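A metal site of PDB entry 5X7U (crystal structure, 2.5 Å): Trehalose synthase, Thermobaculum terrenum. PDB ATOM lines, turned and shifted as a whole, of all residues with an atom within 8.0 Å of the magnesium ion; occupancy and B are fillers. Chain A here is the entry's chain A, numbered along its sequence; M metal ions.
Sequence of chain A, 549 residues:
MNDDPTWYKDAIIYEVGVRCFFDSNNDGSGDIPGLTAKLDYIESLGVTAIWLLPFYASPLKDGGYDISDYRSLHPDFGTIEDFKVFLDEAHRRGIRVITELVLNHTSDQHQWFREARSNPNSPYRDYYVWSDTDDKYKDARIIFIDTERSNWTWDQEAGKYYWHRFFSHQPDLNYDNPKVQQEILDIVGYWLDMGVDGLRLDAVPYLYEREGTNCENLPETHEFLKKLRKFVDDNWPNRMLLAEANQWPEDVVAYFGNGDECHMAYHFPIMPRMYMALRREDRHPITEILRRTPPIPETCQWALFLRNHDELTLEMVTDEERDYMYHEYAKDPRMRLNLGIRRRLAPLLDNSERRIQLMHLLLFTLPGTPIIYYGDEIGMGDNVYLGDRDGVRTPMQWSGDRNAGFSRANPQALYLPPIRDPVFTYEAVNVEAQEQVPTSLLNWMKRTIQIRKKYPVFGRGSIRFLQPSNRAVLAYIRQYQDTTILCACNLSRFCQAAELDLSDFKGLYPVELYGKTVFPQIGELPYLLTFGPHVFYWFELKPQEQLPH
The side-chain carboxylate (OD2) of Asp 23 lies close to the backbone NH (N) of Asn 26. The side-chain carboxylate (OD2) of Asp 23 sits at hydrogen-bond distance from the backbone NH (N) of Gly 28, at 2.8 Å. N of Asp 23 is in hydrogen-bond range of O of Phe 406, 3.1 Å away. OG of Ser 29 sits at hydrogen-bond distance from NE of Arg 19. The side-chain carboxylate (OD1) of Asp 31 sits at hydrogen-bond distance from the side-chain hydroxyl (OG) of Ser 24 (2.4 Å). N of Asp 31 is in hydrogen-bond range of O of Phe 22, 3.1 Å away. The side-chain carboxylate (OD1) of Asp 31 lies within hydrogen-bond range of the backbone NH (N) of Gly 34 (2.8 Å). The backbone NH (N) of Asp 31 sits at hydrogen-bond distance from the backbone carbonyl oxygen (O) of Val 18 (3.5 Å).
Five residues have an atom within 4 Å of the magnesium ion: Asp 23, Asn 25, Asp 27, Ser 29 and Asp 31. The nearest printed residue that does not touch the magnesium ion is Asp 76 (4.1 Å).
The magnesium ion is bound by OD1 of Asp 23. O of Ser 29 binds the magnesium ion (2.3 Å). The side-chain carboxylate (OD2) of Asp 31 is bound to the magnesium ion (2.3 Å). OD1 of Asn 25 binds the magnesium ion (2.3 Å). OD1 of Asp 27 binds the magnesium ion (2.4 Å).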
ATOM      1  N   VAL A  18      22.085  -7.045  18.307  1.00  0.00           N
ATOM      2  CA  VAL A  18      22.053  -5.770  19.027  1.00  0.00           C
ATOM      3  C   VAL A  18      23.395  -5.487  19.677  1.00  0.00           C
ATOM      4  O   VAL A  18      23.898  -4.352  19.640  1.00  0.00           O
ATOM      5  CB  VAL A  18      20.920  -5.781  20.068  1.00  0.00           C
ATOM      6  CG1 VAL A  18      20.913  -4.465  20.835  1.00  0.00           C
ATOM      7  CG2 VAL A  18      19.581  -6.039  19.398  1.00  0.00           C
ATOM      8  N   ARG A  19      23.997  -6.511  20.274  1.00  0.00           N
ATOM      9  CA  ARG A  19      25.266  -6.329  20.972  1.00  0.00           C
ATOM     10  C   ARG A  19      26.389  -5.956  20.031  1.00  0.00           C
ATOM     11  O   ARG A  19      27.379  -5.366  20.470  1.00  0.00           O
ATOM     12  CB  ARG A  19      25.594  -7.601  21.763  1.00  0.00           C
ATOM     13  CG  ARG A  19      26.972  -7.669  22.330  1.00  0.00           C
ATOM     14  CD  ARG A  19      27.047  -8.638  23.484  1.00  0.00           C
ATOM     15  NE  ARG A  19      26.655  -7.907  24.677  1.00  0.00           N
ATOM     16  CZ  ARG A  19      27.241  -8.041  25.859  1.00  0.00           C
ATOM     17  NH1 ARG A  19      28.249  -8.905  26.024  1.00  0.00           N
ATOM     18  NH2 ARG A  19      26.817  -7.295  26.863  1.00  0.00           N
ATOM     19  N   PHE A  22      25.874  -1.015  17.451  1.00  0.00           N
ATOM     20  CA  PHE A  22      26.342   0.310  17.856  1.00  0.00           C
ATOM     21  C   PHE A  22      26.114   0.521  19.345  1.00  0.00           C
ATOM     22  O   PHE A  22      25.006   0.295  19.851  1.00  0.00           O
ATOM     23  CB  PHE A  22      25.640   1.410  17.060  1.00  0.00           C
ATOM     24  CG  PHE A  22      26.199   2.791  17.312  1.00  0.00           C
ATOM     25  CD1 PHE A  22      27.518   3.088  16.981  1.00  0.00           C
ATOM     26  CD2 PHE A  22      25.405   3.790  17.854  1.00  0.00           C
ATOM     27  CE1 PHE A  22      28.048   4.362  17.198  1.00  0.00           C
ATOM     28  CE2 PHE A  22      25.920   5.076  18.081  1.00  0.00           C
ATOM     29  CZ  PHE A  22      27.239   5.360  17.747  1.00  0.00           C
ATOM     30  N   ASP A  23      27.184   0.925  20.035  1.00  0.00           N
ATOM     31  CA  ASP A  23      27.168   1.194  21.466  1.00  0.00           C
ATOM     32  C   ASP A  23      26.871   2.679  21.670  1.00  0.00           C
ATOM     33  O   ASP A  23      27.704   3.534  21.367  1.00  0.00           O
ATOM     34  CB  ASP A  23      28.508   0.818  22.097  1.00  0.00           C
ATOM     35  CG  ASP A  23      28.552   1.065  23.599  1.00  0.00           C
ATOM     36  OD1 ASP A  23      27.480   1.148  24.255  1.00  0.00           O
ATOM     37  OD2 ASP A  23      29.684   1.146  24.126  1.00  0.00           O
ATOM     38  N   SER A  24      25.663   2.989  22.165  1.00  0.00           N
ATOM     39  CA  SER A  24      25.241   4.382  22.306  1.00  0.00           C
ATOM     40  C   SER A  24      25.674   5.033  23.608  1.00  0.00           C
ATOM     41  O   SER A  24      25.836   6.240  23.645  1.00  0.00           O
ATOM     42  CB  SER A  24      23.722   4.496  22.194  1.00  0.00           C
ATOM     43  OG  SER A  24      23.077   3.809  23.260  1.00  0.00           O
ATOM     44  N   ASN A  25      25.850   4.258  24.682  1.00  0.00           N
ATOM     45  CA  ASN A  25      26.290   4.798  25.968  1.00  0.00           C
ATOM     46  C   ASN A  25      27.757   4.502  26.281  1.00  0.00           C
ATOM     47  O   ASN A  25      28.195   4.815  27.394  1.00  0.00           O
ATOM     48  CB  ASN A  25      25.433   4.226  27.090  1.00  0.00           C
ATOM     49  CG  ASN A  25      25.626   2.751  27.224  1.00  0.00           C
ATOM     50  OD1 ASN A  25      26.034   2.075  26.265  1.00  0.00           O
ATOM     51  ND2 ASN A  25      25.332   2.217  28.395  1.00  0.00           N
ATOM     52  N   ASN A  26      28.497   3.857  25.393  1.00  0.00           N
ATOM     53  CA  ASN A  26      29.944   3.726  25.527  1.00  0.00           C
ATOM     54  C   ASN A  26      30.348   2.877  26.734  1.00  0.00           C
ATOM     55  O   ASN A  26      31.328   3.196  27.424  1.00  0.00           O
ATOM     56  CB  ASN A  26      30.621   5.085  25.580  1.00  0.00           C
ATOM     57  CG  ASN A  26      30.290   5.948  24.367  1.00  0.00           C
ATOM     58  OD1 ASN A  26      30.369   5.494  23.220  1.00  0.00           O
ATOM     59  ND2 ASN A  26      29.904   7.189  24.617  1.00  0.00           N
ATOM     60  N   ASP A  27      29.617   1.799  26.989  1.00  0.00           N
ATOM     61  CA  ASP A  27      29.995   0.812  27.983  1.00  0.00           C
ATOM     62  C   ASP A  27      30.680  -0.411  27.381  1.00  0.00           C
ATOM     63  O   ASP A  27      30.984  -1.367  28.099  1.00  0.00           O
ATOM     64  CB  ASP A  27      28.773   0.371  28.797  1.00  0.00           C
ATOM     65  CG  ASP A  27      27.671  -0.250  27.927  1.00  0.00           C
ATOM     66  OD1 ASP A  27      27.824  -0.272  26.701  1.00  0.00           O
ATOM     67  OD2 ASP A  27      26.645  -0.693  28.466  1.00  0.00           O
ATOM     68  N   GLY A  28      30.918  -0.411  26.067  1.00  0.00           N
ATOM     69  CA  GLY A  28      31.568  -1.515  25.408  1.00  0.00           C
ATOM     70  C   GLY A  28      30.639  -2.499  24.727  1.00  0.00           C
ATOM     71  O   GLY A  28      31.118  -3.415  24.045  1.00  0.00           O
ATOM     72  N   SER A  29      29.329  -2.323  24.877  1.00  0.00           N
ATOM     73  CA  SER A  29      28.374  -3.246  24.299  1.00  0.00           C
ATOM     74  C   SER A  29      27.355  -2.506  23.456  1.00  0.00           C
ATOM     75  O   SER A  29      26.858  -1.441  23.849  1.00  0.00           O
ATOM     76  CB  SER A  29      27.673  -4.036  25.381  1.00  0.00           C
ATOM     77  OG  SER A  29      26.510  -4.621  24.861  1.00  0.00           O
ATOM     78  N   GLY A  30      27.031  -3.063  22.290  1.00  0.00           N
ATOM     79  CA  GLY A  30      25.965  -2.497  21.496  1.00  0.00           C
ATOM     80  C   GLY A  30      24.628  -2.563  22.205  1.00  0.00           C
ATOM     81  O   GLY A  30      24.405  -3.407  23.071  1.00  0.00           O
ATOM     82  N   ASP A  31      23.722  -1.650  21.844  1.00  0.00           N
ATOM     83  CA  ASP A  31      22.445  -1.591  22.535  1.00  0.00           C
ATOM     84  C   ASP A  31      21.339  -1.141  21.598  1.00  0.00           C
ATOM     85  O   ASP A  31      21.573  -0.660  20.483  1.00  0.00           O
ATOM     86  CB  ASP A  31      22.522  -0.654  23.735  1.00  0.00           C
ATOM     87  CG  ASP A  31      23.186   0.656  23.401  1.00  0.00           C
ATOM     88  OD1 ASP A  31      22.524   1.498  22.746  1.00  0.00           O
ATOM     89  OD2 ASP A  31      24.369   0.833  23.793  1.00  0.00           O
ATOM     90  N   ILE A  32      20.101  -1.296  22.084  1.00  0.00           N
ATOM     91  CA  ILE A  32      18.930  -0.960  21.263  1.00  0.00           C
ATOM     92  C   ILE A  32      18.864   0.507  20.895  1.00  0.00           C
ATOM     93  O   ILE A  32      18.619   0.815  19.715  1.00  0.00           O
ATOM     94  CB  ILE A  32      17.657  -1.469  21.945  1.00  0.00           C
ATOM     95  CG1 ILE A  32      17.663  -2.988  21.949  1.00  0.00           C
ATOM     96  CG2 ILE A  32      16.416  -0.940  21.251  1.00  0.00           C
ATOM     97  CD1 ILE A  32      16.367  -3.585  22.339  1.00  0.00           C
ATOM     98  N   PRO A  33      19.073   1.470  21.796  1.00  0.00           N
ATOM     99  CA  PRO A  33      19.117   2.873  21.339  1.00  0.00           C
ATOM    100  C   PRO A  33      20.197   3.121  20.302  1.00  0.00           C
ATOM    101  O   PRO A  33      20.014   3.937  19.396  1.00  0.00           O
ATOM    102  CB  PRO A  33      19.373   3.665  22.640  1.00  0.00           C
ATOM    103  CG  PRO A  33      18.914   2.750  23.754  1.00  0.00           C
ATOM    104  CD  PRO A  33      19.205   1.361  23.268  1.00  0.00           C
ATOM    105  N   GLY A  34      21.344   2.430  20.420  1.00  0.00           N
ATOM    106  CA  GLY A  34      22.363   2.557  19.384  1.00  0.00           C
ATOM    107  C   GLY A  34      21.886   1.997  18.057  1.00  0.00           C
ATOM    108  O   GLY A  34      22.105   2.604  16.997  1.00  0.00           O
ATOM    109  N   PRO A  75      20.122  -6.530  30.400  1.00  0.00           N
ATOM    110  CA  PRO A  75      20.384  -5.143  30.839  1.00  0.00           C
ATOM    111  C   PRO A  75      21.313  -4.354  29.928  1.00  0.00           C
ATOM    112  O   PRO A  75      21.161  -3.137  29.828  1.00  0.00           O
ATOM    113  CB  PRO A  75      21.009  -5.332  32.232  1.00  0.00           C
ATOM    114  CG  PRO A  75      20.636  -6.700  32.648  1.00  0.00           C
ATOM    115  CD  PRO A  75      20.495  -7.523  31.423  1.00  0.00           C
ATOM    116  N   ASP A  76      22.279  -4.997  29.276  1.00  0.00           N
ATOM    117  CA  ASP A  76      23.179  -4.231  28.411  1.00  0.00           C
ATOM    118  C   ASP A  76      22.501  -3.675  27.177  1.00  0.00           C
ATOM    119  O   ASP A  76      23.059  -2.777  26.527  1.00  0.00           O
ATOM    120  CB  ASP A  76      24.363  -5.087  27.985  1.00  0.00           C
ATOM    121  CG  ASP A  76      25.204  -5.515  29.137  1.00  0.00           C
ATOM    122  OD1 ASP A  76      26.184  -6.269  28.918  1.00  0.00           O
ATOM    123  OD2 ASP A  76      24.882  -5.106  30.278  1.00  0.00           O
ATOM    124  N   PHE A  77      21.322  -4.187  26.808  1.00  0.00           N
ATOM    125  CA  PHE A  77      20.679  -3.794  25.557  1.00  0.00           C
ATOM    126  C   PHE A  77      19.584  -2.750  25.738  1.00  0.00           C
ATOM    127  O   PHE A  77      19.145  -2.171  24.743  1.00  0.00           O
ATOM    128  CB  PHE A  77      20.105  -5.016  24.846  1.00  0.00           C
ATOM    129  CG  PHE A  77      21.118  -6.089  24.598  1.00  0.00           C
ATOM    130  CD1 PHE A  77      22.479  -5.781  24.506  1.00  0.00           C
ATOM    131  CD2 PHE A  77      20.722  -7.413  24.440  1.00  0.00           C
ATOM    132  CE1 PHE A  77      23.425  -6.777  24.274  1.00  0.00           C
ATOM    133  CE2 PHE A  77      21.658  -8.421  24.200  1.00  0.00           C
ATOM    134  CZ  PHE A  77      23.000  -8.108  24.123  1.00  0.00           C
ATOM    135  N   GLY A  78      19.164  -2.485  26.963  1.00  0.00           N
ATOM    136  CA  GLY A  78      18.149  -1.481  27.198  1.00  0.00           C
ATOM    137  C   GLY A  78      16.897  -2.042  27.850  1.00  0.00           C
ATOM    138  O   GLY A  78      16.917  -3.114  28.453  1.00  0.00           O
ATOM    139  N   PHE A 406      32.533   1.994  16.603  1.00  0.00           N
ATOM    140  CA  PHE A 406      31.435   1.276  17.233  1.00  0.00           C
ATOM    141  C   PHE A 406      31.166   1.775  18.651  1.00  0.00           C
ATOM    142  O   PHE A 406      30.051   1.605  19.163  1.00  0.00           O
ATOM    143  CB  PHE A 406      31.757  -0.227  17.230  1.00  0.00           C
ATOM    144  CG  PHE A 406      31.054  -1.027  18.292  1.00  0.00           C
ATOM    145  CD1 PHE A 406      29.752  -1.511  18.089  1.00  0.00           C
ATOM    146  CD2 PHE A 406      31.690  -1.352  19.486  1.00  0.00           C
ATOM    147  CE1 PHE A 406      29.117  -2.273  19.057  1.00  0.00           C
ATOM    148  CE2 PHE A 406      31.052  -2.108  20.461  1.00  0.00           C
ATOM    149  CZ  PHE A 406      29.769  -2.583  20.246  1.00  0.00           C
ATOM    150  N   SER A 407      32.142   2.402  19.270  1.00  0.00           N
ATOM    151  CA  SER A 407      32.057   2.749  20.676  1.00  0.00           C
ATOM    152  C   SER A 407      33.136   3.771  20.987  1.00  0.00           C
ATOM    153  O   SER A 407      34.149   3.863  20.288  1.00  0.00           O
ATOM    154  CB  SER A 407      32.211   1.512  21.563  1.00  0.00           C
ATOM    155  OG  SER A 407      32.106   1.837  22.937  1.00  0.00           O
HETATM  156 MG    MG M   1      25.888  -0.005  25.291  1.00  0.00          MG
